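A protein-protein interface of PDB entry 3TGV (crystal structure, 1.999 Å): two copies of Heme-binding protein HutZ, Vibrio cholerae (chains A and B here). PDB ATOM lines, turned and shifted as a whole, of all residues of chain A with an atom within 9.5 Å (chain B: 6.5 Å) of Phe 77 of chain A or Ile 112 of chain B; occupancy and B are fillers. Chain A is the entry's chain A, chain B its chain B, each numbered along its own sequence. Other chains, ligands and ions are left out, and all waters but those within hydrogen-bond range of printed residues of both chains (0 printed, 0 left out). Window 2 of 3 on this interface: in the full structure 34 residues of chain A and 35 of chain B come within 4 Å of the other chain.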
ATOM      1  N   ILE A  67     -16.047  23.280  20.975  1.00  0.00           N
ATOM      2  CA  ILE A  67     -17.124  24.263  20.841  1.00  0.00           C
ATOM      3  C   ILE A  67     -17.601  24.873  22.168  1.00  0.00           C
ATOM      4  O   ILE A  67     -17.636  24.191  23.204  1.00  0.00           O
ATOM      5  CB  ILE A  67     -18.337  23.642  20.087  1.00  0.00           C
ATOM      6  CG1 ILE A  67     -19.400  24.704  19.819  1.00  0.00           C
ATOM      7  CG2 ILE A  67     -18.910  22.426  20.865  1.00  0.00           C
ATOM      8  CD1 ILE A  67     -20.375  24.309  18.736  1.00  0.00           C
ATOM      9  N   GLU A  68     -17.963  26.156  22.148  1.00  0.00           N
ATOM     10  CA  GLU A  68     -18.441  26.795  23.369  1.00  0.00           C
ATOM     11  C   GLU A  68     -19.828  26.256  23.698  1.00  0.00           C
ATOM     12  O   GLU A  68     -20.515  25.740  22.824  1.00  0.00           O
ATOM     13  CB  GLU A  68     -18.484  28.323  23.246  1.00  0.00           C
ATOM     14  CG  GLU A  68     -19.655  28.850  22.450  1.00  0.00           C
ATOM     15  CD  GLU A  68     -19.626  30.373  22.302  1.00  0.00           C
ATOM     16  OE1 GLU A  68     -19.111  31.071  23.201  1.00  0.00           O
ATOM     17  OE2 GLU A  68     -20.127  30.863  21.285  1.00  0.00           O
ATOM     18  N   GLU A  70     -23.829  25.856  24.692  1.00  0.00           N
ATOM     19  CA  GLU A  70     -25.042  26.516  24.236  1.00  0.00           C
ATOM     20  C   GLU A  70     -25.351  27.730  25.099  1.00  0.00           C
ATOM     21  O   GLU A  70     -25.655  28.796  24.578  1.00  0.00           O
ATOM     22  CB  GLU A  70     -26.251  25.573  24.240  1.00  0.00           C
ATOM     23  CG  GLU A  70     -26.390  24.743  22.991  1.00  0.00           C
ATOM     24  CD  GLU A  70     -27.627  23.884  22.987  1.00  0.00           C
ATOM     25  OE1 GLU A  70     -28.670  24.327  23.523  1.00  0.00           O
ATOM     26  OE2 GLU A  70     -27.548  22.747  22.473  1.00  0.00           O
ATOM     27  N   ALA A  73     -23.094  30.890  24.461  1.00  0.00           N
ATOM     28  CA  ALA A  73     -23.078  31.496  23.130  1.00  0.00           C
ATOM     29  C   ALA A  73     -23.943  32.749  23.013  1.00  0.00           C
ATOM     30  O   ALA A  73     -25.134  32.730  23.333  1.00  0.00           O
ATOM     31  CB  ALA A  73     -23.482  30.487  22.081  1.00  0.00           C
ATOM     32  N   LYS A  74     -23.331  33.827  22.534  1.00  0.00           N
ATOM     33  CA  LYS A  74     -24.044  35.052  22.205  1.00  0.00           C
ATOM     34  C   LYS A  74     -25.037  34.753  21.094  1.00  0.00           C
ATOM     35  O   LYS A  74     -26.205  35.140  21.168  1.00  0.00           O
ATOM     36  CB  LYS A  74     -23.062  36.127  21.741  1.00  0.00           C
ATOM     37  CG  LYS A  74     -23.030  37.393  22.592  1.00  0.00           C
ATOM     38  CD  LYS A  74     -21.935  38.344  22.096  1.00  0.00           C
ATOM     39  CE  LYS A  74     -22.137  39.774  22.598  1.00  0.00           C
ATOM     40  NZ  LYS A  74     -21.081  40.701  22.088  1.00  0.00           N
ATOM     41  N   GLN A  75     -24.574  34.051  20.064  1.00  0.00           N
ATOM     42  CA  GLN A  75     -25.448  33.706  18.950  1.00  0.00           C
ATOM     43  C   GLN A  75     -25.523  32.208  18.726  1.00  0.00           C
ATOM     44  O   GLN A  75     -24.542  31.591  18.318  1.00  0.00           O
ATOM     45  CB  GLN A  75     -24.952  34.357  17.665  1.00  0.00           C
ATOM     46  CG  GLN A  75     -25.499  33.672  16.421  1.00  0.00           C
ATOM     47  CD  GLN A  75     -26.972  33.961  16.207  1.00  0.00           C
ATOM     48  OE1 GLN A  75     -27.835  33.152  16.530  1.00  0.00           O
ATOM     49  NE2 GLN A  75     -27.262  35.134  15.649  1.00  0.00           N
ATOM     50  N   LEU A  76     -26.692  31.626  18.954  1.00  0.00           N
ATOM     51  CA  LEU A  76     -26.851  30.179  18.796  1.00  0.00           C
ATOM     52  C   LEU A  76     -26.486  29.685  17.399  1.00  0.00           C
ATOM     53  O   LEU A  76     -25.965  28.589  17.247  1.00  0.00           O
ATOM     54  CB  LEU A  76     -28.264  29.732  19.164  1.00  0.00           C
ATOM     55  CG  LEU A  76     -28.442  29.499  20.659  1.00  0.00           C
ATOM     56  CD1 LEU A  76     -29.855  29.009  20.926  1.00  0.00           C
ATOM     57  CD2 LEU A  76     -27.406  28.508  21.183  1.00  0.00           C
ATOM     58  N   PHE A  77     -26.745  30.499  16.378  1.00  0.00           N
ATOM     59  CA  PHE A  77     -26.378  30.126  15.014  1.00  0.00           C
ATOM     60  C   PHE A  77     -24.899  30.369  14.690  1.00  0.00           C
ATOM     61  O   PHE A  77     -24.449  30.102  13.583  1.00  0.00           O
ATOM     62  CB  PHE A  77     -27.298  30.808  13.993  1.00  0.00           C
ATOM     63  CG  PHE A  77     -28.631  30.141  13.866  1.00  0.00           C
ATOM     64  CD1 PHE A  77     -29.628  30.380  14.793  1.00  0.00           C
ATOM     65  CD2 PHE A  77     -28.869  29.238  12.845  1.00  0.00           C
ATOM     66  CE1 PHE A  77     -30.850  29.745  14.690  1.00  0.00           C
ATOM     67  CE2 PHE A  77     -30.083  28.611  12.722  1.00  0.00           C
ATOM     68  CZ  PHE A  77     -31.080  28.858  13.645  1.00  0.00           C
ATOM     69  N   ALA A  78     -24.155  30.855  15.676  1.00  0.00           N
ATOM     70  CA  ALA A  78     -22.729  31.111  15.520  1.00  0.00           C
ATOM     71  C   ALA A  78     -21.986  30.786  16.810  1.00  0.00           C
ATOM     72  O   ALA A  78     -21.407  31.662  17.451  1.00  0.00           O
ATOM     73  CB  ALA A  78     -22.486  32.570  15.109  1.00  0.00           C
ATOM     74  N   ARG A  79     -22.025  29.522  17.210  1.00  0.00           N
ATOM     75  CA  ARG A  79     -21.266  29.082  18.371  1.00  0.00           C
ATOM     76  C   ARG A  79     -19.770  29.142  18.055  1.00  0.00           C
ATOM     77  O   ARG A  79     -19.306  28.646  17.030  1.00  0.00           O
ATOM     78  CB  ARG A  79     -21.712  27.681  18.827  1.00  0.00           C
ATOM     79  CG  ARG A  79     -23.112  27.644  19.459  1.00  0.00           C
ATOM     80  CD  ARG A  79     -23.600  26.220  19.709  1.00  0.00           C
ATOM     81  NE  ARG A  79     -22.930  25.594  20.841  1.00  0.00           N
ATOM     82  CZ  ARG A  79     -23.043  24.311  21.170  1.00  0.00           C
ATOM     83  NH1 ARG A  79     -23.810  23.488  20.459  1.00  0.00           N
ATOM     84  NH2 ARG A  79     -22.389  23.847  22.221  1.00  0.00           N
ATOM     85  N   LYS A  80     -19.023  29.798  18.929  1.00  0.00           N
ATOM     86  CA  LYS A  80     -17.576  29.890  18.801  1.00  0.00           C
ATOM     87  C   LYS A  80     -16.991  28.483  18.790  1.00  0.00           C
ATOM     88  O   LYS A  80     -17.286  27.675  19.679  1.00  0.00           O
ATOM     89  CB  LYS A  80     -17.035  30.697  19.986  1.00  0.00           C
ATOM     90  CG  LYS A  80     -15.555  30.983  20.008  1.00  0.00           C
ATOM     91  CD  LYS A  80     -15.266  32.030  21.093  1.00  0.00           C
ATOM     92  CE  LYS A  80     -13.835  31.984  21.586  1.00  0.00           C
ATOM     93  NZ  LYS A  80     -13.584  32.897  22.749  1.00  0.00           N
ATOM     94  N   ARG A  81     -16.173  28.176  17.787  1.00  0.00           N
ATOM     95  CA  ARG A  81     -15.690  26.808  17.634  1.00  0.00           C
ATOM     96  C   ARG A  81     -14.420  26.675  16.803  1.00  0.00           C
ATOM     97  O   ARG A  81     -14.096  27.553  15.994  1.00  0.00           O
ATOM     98  CB  ARG A  81     -16.788  25.944  17.015  1.00  0.00           C
ATOM     99  CG  ARG A  81     -17.169  26.338  15.586  1.00  0.00           C
ATOM    100  CD  ARG A  81     -18.503  25.707  15.190  1.00  0.00           C
ATOM    101  NE  ARG A  81     -18.860  25.979  13.801  1.00  0.00           N
ATOM    102  CZ  ARG A  81     -19.576  27.029  13.398  1.00  0.00           C
ATOM    103  NH1 ARG A  81     -20.023  27.912  14.277  1.00  0.00           N
ATOM    104  NH2 ARG A  81     -19.847  27.192  12.110  1.00  0.00           N
ATOM    105  N   PHE A 134     -10.344  25.018  10.989  1.00  0.00           N
ATOM    106  CA  PHE A 134     -11.331  26.072  10.815  1.00  0.00           C
ATOM    107  C   PHE A 134     -11.633  26.704  12.160  1.00  0.00           C
ATOM    108  O   PHE A 134     -11.818  26.012  13.166  1.00  0.00           O
ATOM    109  CB  PHE A 134     -12.597  25.520  10.193  1.00  0.00           C
ATOM    110  CG  PHE A 134     -13.722  26.515  10.110  1.00  0.00           C
ATOM    111  CD1 PHE A 134     -14.809  26.425  10.965  1.00  0.00           C
ATOM    112  CD2 PHE A 134     -13.717  27.509   9.148  1.00  0.00           C
ATOM    113  CE1 PHE A 134     -15.859  27.338  10.878  1.00  0.00           C
ATOM    114  CE2 PHE A 134     -14.754  28.421   9.057  1.00  0.00           C
ATOM    115  CZ  PHE A 134     -15.834  28.327   9.923  1.00  0.00           C
ATOM    116  N   LYS A 136     -13.973  29.713  14.087  1.00  0.00           N
ATOM    117  CA  LYS A 136     -15.120  30.600  13.954  1.00  0.00           C
ATOM    118  C   LYS A 136     -15.424  31.326  15.265  1.00  0.00           C
ATOM    119  O   LYS A 136     -15.484  30.698  16.328  1.00  0.00           O
ATOM    120  CB  LYS A 136     -16.341  29.810  13.477  1.00  0.00           C
ATOM    121  CG  LYS A 136     -17.617  30.627  13.399  1.00  0.00           C
ATOM    122  CD  LYS A 136     -17.718  31.397  12.087  1.00  0.00           C
ATOM    123  CE  LYS A 136     -19.076  32.078  11.948  1.00  0.00           C
ATOM    124  NZ  LYS A 136     -18.965  33.543  12.203  1.00  0.00           N
ATOM    125  N   GLY A 137     -15.588  32.644  15.183  1.00  0.00           N
ATOM    126  CA  GLY A 137     -15.993  33.457  16.320  1.00  0.00           C
ATOM    127  C   GLY A 137     -14.889  34.053  17.175  1.00  0.00           C
ATOM    128  O   GLY A 137     -15.143  34.494  18.301  1.00  0.00           O
ATOM    129  N   TYR B  32     -22.689  21.150  14.156  1.00  0.00           N
ATOM    130  CA  TYR B  32     -23.862  21.298  15.021  1.00  0.00           C
ATOM    131  C   TYR B  32     -24.888  22.130  14.281  1.00  0.00           C
ATOM    132  O   TYR B  32     -24.556  22.811  13.313  1.00  0.00           O
ATOM    133  CB  TYR B  32     -23.507  22.006  16.335  1.00  0.00           C
ATOM    134  CG  TYR B  32     -23.582  23.517  16.227  1.00  0.00           C
ATOM    135  CD1 TYR B  32     -22.524  24.250  15.708  1.00  0.00           C
ATOM    136  CD2 TYR B  32     -24.724  24.204  16.626  1.00  0.00           C
ATOM    137  CE1 TYR B  32     -22.597  25.642  15.584  1.00  0.00           C
ATOM    138  CE2 TYR B  32     -24.804  25.584  16.514  1.00  0.00           C
ATOM    139  CZ  TYR B  32     -23.741  26.293  15.997  1.00  0.00           C
ATOM    140  OH  TYR B  32     -23.823  27.659  15.897  1.00  0.00           O
ATOM    141  N   ALA B  33     -26.129  22.095  14.742  1.00  0.00           N
ATOM    142  CA  ALA B  33     -27.139  22.993  14.202  1.00  0.00           C
ATOM    143  C   ALA B  33     -28.297  23.135  15.178  1.00  0.00           C
ATOM    144  O   ALA B  33     -28.721  22.148  15.788  1.00  0.00           O
ATOM    145  CB  ALA B  33     -27.638  22.487  12.856  1.00  0.00           C
ATOM    146  N   PRO B  34     -28.806  24.367  15.331  1.00  0.00           N
ATOM    147  CA  PRO B  34     -30.092  24.589  16.010  1.00  0.00           C
ATOM    148  C   PRO B  34     -31.160  23.708  15.362  1.00  0.00           C
ATOM    149  O   PRO B  34     -31.120  23.495  14.148  1.00  0.00           O
ATOM    150  CB  PRO B  34     -30.406  26.058  15.705  1.00  0.00           C
ATOM    151  CG  PRO B  34     -29.057  26.687  15.428  1.00  0.00           C
ATOM    152  CD  PRO B  34     -28.200  25.616  14.819  1.00  0.00           C
ATOM    153  N   PHE B  35     -32.101  23.209  16.148  1.00  0.00           N
ATOM    154  CA  PHE B  35     -33.151  22.358  15.607  1.00  0.00           C
ATOM    155  C   PHE B  35     -34.504  22.730  16.166  1.00  0.00           C
ATOM    156  O   PHE B  35     -34.595  23.414  17.184  1.00  0.00           O
ATOM    157  CB  PHE B  35     -32.880  20.904  15.990  1.00  0.00           C
ATOM    158  CG  PHE B  35     -33.191  20.589  17.433  1.00  0.00           C
ATOM    159  CD1 PHE B  35     -32.254  20.819  18.421  1.00  0.00           C
ATOM    160  CD2 PHE B  35     -34.416  20.070  17.798  1.00  0.00           C
ATOM    161  CE1 PHE B  35     -32.529  20.532  19.742  1.00  0.00           C
ATOM    162  CE2 PHE B  35     -34.699  19.773  19.125  1.00  0.00           C
ATOM    163  CZ  PHE B  35     -33.757  20.004  20.096  1.00  0.00           C
ATOM    164  N   LEU B  45     -31.772  23.854   9.777  1.00  0.00           N
ATOM    165  CA  LEU B  45     -31.679  24.782   8.658  1.00  0.00           C
ATOM    166  C   LEU B  45     -30.210  25.159   8.492  1.00  0.00           C
ATOM    167  O   LEU B  45     -29.669  25.910   9.301  1.00  0.00           O
ATOM    168  CB  LEU B  45     -32.503  26.036   8.973  1.00  0.00           C
ATOM    169  CG  LEU B  45     -32.469  27.147   7.922  1.00  0.00           C
ATOM    170  CD1 LEU B  45     -33.195  26.679   6.667  1.00  0.00           C
ATOM    171  CD2 LEU B  45     -33.120  28.398   8.473  1.00  0.00           C
ATOM    172  N   MET B 105     -39.471  27.308  13.688  1.00  0.00           N
ATOM    173  CA  MET B 105     -38.115  27.795  13.954  1.00  0.00           C
ATOM    174  C   MET B 105     -38.064  29.252  14.358  1.00  0.00           C
ATOM    175  O   MET B 105     -37.348  29.624  15.292  1.00  0.00           O
ATOM    176  CB  MET B 105     -37.235  27.602  12.723  1.00  0.00           C
ATOM    177  CG  MET B 105     -37.098  26.146  12.344  1.00  0.00           C
ATOM    178  SD  MET B 105     -35.543  25.785  11.534  1.00  0.00           S
ATOM    179  CE  MET B 105     -36.011  25.790   9.818  1.00  0.00           C
ATOM    180  N   PHE B 109     -36.421  30.505  17.694  1.00  0.00           N
ATOM    181  CA  PHE B 109     -35.131  31.178  17.545  1.00  0.00           C
ATOM    182  C   PHE B 109     -35.214  32.681  17.253  1.00  0.00           C
ATOM    183  O   PHE B 109     -34.232  33.403  17.406  1.00  0.00           O
ATOM    184  CB  PHE B 109     -34.284  30.449  16.494  1.00  0.00           C
ATOM    185  CG  PHE B 109     -33.925  29.045  16.910  1.00  0.00           C
ATOM    186  CD1 PHE B 109     -33.077  28.833  17.978  1.00  0.00           C
ATOM    187  CD2 PHE B 109     -34.468  27.946  16.262  1.00  0.00           C
ATOM    188  CE1 PHE B 109     -32.765  27.541  18.390  1.00  0.00           C
ATOM    189  CE2 PHE B 109     -34.161  26.646  16.671  1.00  0.00           C
ATOM    190  CZ  PHE B 109     -33.307  26.451  17.731  1.00  0.00           C
ATOM    191  N   GLY B 110     -36.387  33.154  16.860  1.00  0.00           N
ATOM    192  CA  GLY B 110     -36.572  34.582  16.686  1.00  0.00           C
ATOM    193  C   GLY B 110     -36.270  35.059  15.275  1.00  0.00           C
ATOM    194  O   GLY B 110     -36.227  34.260  14.340  1.00  0.00           O
ATOM    195  N   GLU B 111     -36.050  36.367  15.135  1.00  0.00           N
ATOM    196  CA  GLU B 111     -35.947  37.020  13.830  1.00  0.00           C
ATOM    197  C   GLU B 111     -34.797  36.503  12.964  1.00  0.00           C
ATOM    198  O   GLU B 111     -34.869  36.575  11.731  1.00  0.00           O
ATOM    199  CB  GLU B 111     -35.832  38.542  14.012  1.00  0.00           C
ATOM    200  CG  GLU B 111     -36.688  39.366  13.044  1.00  0.00           C
ATOM    201  CD  GLU B 111     -35.965  39.752  11.750  1.00  0.00           C
ATOM    202  OE1 GLU B 111     -36.561  40.498  10.926  1.00  0.00           O
ATOM    203  OE2 GLU B 111     -34.804  39.315  11.554  1.00  0.00           O
ATOM    204  N   ILE B 112     -33.747  35.970  13.593  1.00  0.00           N
ATOM    205  CA  ILE B 112     -32.625  35.441  12.821  1.00  0.00           C
ATOM    206  C   ILE B 112     -33.167  34.561  11.705  1.00  0.00           C
ATOM    207  O   ILE B 112     -32.634  34.545  10.595  1.00  0.00           O
ATOM    208  CB  ILE B 112     -31.623  34.650  13.699  1.00  0.00           C
ATOM    209  CG1 ILE B 112     -30.390  34.245  12.898  1.00  0.00           C
ATOM    210  CG2 ILE B 112     -32.270  33.385  14.279  1.00  0.00           C
ATOM    211  CD1 ILE B 112     -29.868  35.330  12.020  1.00  0.00           C
ATOM    212  N   ILE B 113     -34.265  33.865  11.995  1.00  0.00           N
ATOM    213  CA  ILE B 113     -34.866  32.958  11.014  1.00  0.00           C
ATOM    214  C   ILE B 113     -35.397  33.676   9.760  1.00  0.00           C
ATOM    215  O   ILE B 113     -35.399  33.115   8.663  1.00  0.00           O
ATOM    216  CB  ILE B 113     -35.983  32.113  11.645  1.00  0.00           C
ATOM    217  CG1 ILE B 113     -35.401  31.254  12.763  1.00  0.00           C
ATOM    218  CG2 ILE B 113     -36.647  31.218  10.606  1.00  0.00           C
ATOM    219  CD1 ILE B 113     -34.304  30.334  12.266  1.00  0.00           C
ATOM    220  N   ASP B 114     -35.849  34.912   9.925  1.00  0.00           N
ATOM    221  CA  ASP B 114     -36.377  35.659   8.787  1.00  0.00           C
ATOM    222  C   ASP B 114     -35.306  35.803   7.720  1.00  0.00           C
ATOM    223  O   ASP B 114     -35.578  35.660   6.530  1.00  0.00           O
ATOM    224  CB  ASP B 114     -36.865  37.042   9.218  1.00  0.00           C
ATOM    225  CG  ASP B 114     -38.146  36.983  10.022  1.00  0.00           C
ATOM    226  OD1 ASP B 114     -38.787  35.911  10.032  1.00  0.00           O
ATOM    227  OD2 ASP B 114     -38.515  38.008  10.638  1.00  0.00           O
ATOM    228  N   GLY B 115     -34.084  36.080   8.158  1.00  0.00           N
ATOM    229  CA  GLY B 115     -32.975  36.251   7.237  1.00  0.00           C
ATOM    230  C   GLY B 115     -32.486  34.943   6.638  1.00  0.00           C
ATOM    231  O   GLY B 115     -32.357  34.824   5.415  1.00  0.00           O
ATOM    232  N   LEU B 116     -32.204  33.958   7.487  1.00  0.00           N
ATOM    233  CA  LEU B 116     -31.658  32.699   6.988  1.00  0.00           C
ATOM    234  C   LEU B 116     -32.602  32.026   5.998  1.00  0.00           C
ATOM    235  O   LEU B 116     -32.170  31.466   4.989  1.00  0.00           O
ATOM    236  CB  LEU B 116     -31.332  31.742   8.140  1.00  0.00           C
ATOM    237  CG  LEU B 116     -30.371  32.281   9.196  1.00  0.00           C
ATOM    238  CD1 LEU B 116     -30.159  31.245  10.305  1.00  0.00           C
ATOM    239  CD2 LEU B 116     -29.045  32.674   8.567  1.00  0.00           C
ATOM    240  N   SER B 117     -33.893  32.078   6.293  1.00  0.00           N
ATOM    241  CA  SER B 117     -34.881  31.394   5.478  1.00  0.00           C
ATOM    242  C   SER B 117     -34.948  31.981   4.072  1.00  0.00           C
ATOM    243  O   SER B 117     -35.572  31.394   3.181  1.00  0.00           O
ATOM    244  CB  SER B 117     -36.255  31.465   6.138  1.00  0.00           C
ATOM    245  OG  SER B 117     -36.652  32.812   6.324  1.00  0.00           O
ATOM    246  N   PHE B 122     -29.105  28.430   2.305  1.00  0.00           N
ATOM    247  CA  PHE B 122     -29.659  27.730   3.467  1.00  0.00           C
ATOM    248  C   PHE B 122     -30.748  26.726   3.118  1.00  0.00           C
ATOM    249  O   PHE B 122     -31.746  27.065   2.496  1.00  0.00           O
ATOM    250  CB  PHE B 122     -30.128  28.710   4.536  1.00  0.00           C
ATOM    251  CG  PHE B 122     -29.047  29.084   5.497  1.00  0.00           C
ATOM    252  CD1 PHE B 122     -28.122  30.063   5.168  1.00  0.00           C
ATOM    253  CD2 PHE B 122     -28.932  28.436   6.721  1.00  0.00           C
ATOM    254  CE1 PHE B 122     -27.107  30.399   6.042  1.00  0.00           C
ATOM    255  CE2 PHE B 122     -27.928  28.775   7.597  1.00  0.00           C
ATOM    256  CZ  PHE B 122     -27.012  29.760   7.259  1.00  0.00           C
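Printed residues of chain A that touch a printed residue of chain B: Ile 67, Leu 76, Phe 77, Ala 78, Arg 79 and Arg 81. Along chain B the printed residues that touch a printed residue of chain A span positions 32 to 116.
N of Lys 136 of chain A sits at hydrogen-bond distance from O of Arg 81 of chain A, at 2.9 Å. O of Arg 79 of chain A lies within hydrogen-bond range of NH1 of Arg 81 of chain A, at 2.9 Å. The side-chain hydroxyl (OG) of Ser 117 of chain B sits at hydrogen-bond distance from the backbone carbonyl oxygen (O) of Ile 113 of chain B, at 2.7 Å. The side-chain amide oxygen (OE1) of Gln 75 of chain A is in hydrogen-bond range of the backbone NH (N) of Phe 77 of chain A, at 2.9 Å. The guanidinium group of Arg 79 of chain A sits at hydrogen-bond distance from the backbone carbonyl oxygen of Glu 68 of chain A, 2.7 Å away.
Tyr 32 of chain B touches Ile 67 of chain A (CD1 to CD1, 3.7 Å). Phe 77 of chain A touches Pro 34 of chain B (CZ to CG, 3.5 Å). Phe 77 of chain A touches Phe 109 of chain B. CE1 of Phe 77 of chain A touches CG2 of Ile 112 of chain B, at 3.9 Å. Phe 77 of chain A touches Ile 113 of chain B (CZ to CD1, 3.8 Å). Phe 77 of chain A touches Leu 116 of chain B. NH1 of Arg 81 of chain A touches CE1 of Tyr 32 of chain B, at 3.7 Å.
The backbone NH (N) of Arg 79 of chain A lies within hydrogen-bond range of the side-chain hydroxyl (OH) of Tyr 32 of chain B (2.9 Å). The backbone NH of Ala 78 of chain A sits at hydrogen-bond distance from the side-chain hydroxyl of Tyr 32 of chain B (3.2 Å). OH of Tyr 32 of chain B sits close to O of Phe 77 of chain A (3.4 Å). The backbone carbonyl oxygen (O) of Leu 76 of chain A is in hydrogen-bond range of the side-chain hydroxyl (OH) of Tyr 32 of chain B (2.7 Å).
No position is printed for both chains.
Of the printed residues of chain B, Leu 76 of chain A touches Tyr 32. Phe 77 of chain A touches just these residues of chain B: Tyr 32 (3.2 Å), Pro 34 (3.5 Å), Phe 109 (3.9 Å), Ile 112 (3.9 Å), Ile 113 (3.8 Å) and Leu 116 (3.5 Å). Printed residues of chain B within 4 Å of Ala 78 of chain A: Tyr 32. Printed residues of chain B within 4 Å of Arg 79 of chain A: Tyr 32 (2.9 Å). Lys 80 of chain A touches none of the printed residues of chain B. Of the printed residues of chain A, Tyr 32 of chain B touches Ile 67, Leu 76, Phe 77, Ala 78, Arg 79 and Arg 81. Ala 33 of chain B touches none of the printed residues of chain A. Of chain A, only Phe 77 (3.5 Å) comes within 4 Å of Pro 34 of chain B. No residue of chain A comes within 4 Å of Gly 110 of chain B. Of chain A, only Phe 77 (3.9 Å) comes within 4 Å of Ile 112 of chain B. Ile 113 of chain B touches just one residue of chain A: Phe 77. Printed residues of chain A within 4 Å of Leu 116 of chain B: Phe 77. The nearest printed residue of chain B that does not touch Leu 76 of chain A is Pro 34 of chain B (4.1 Å).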
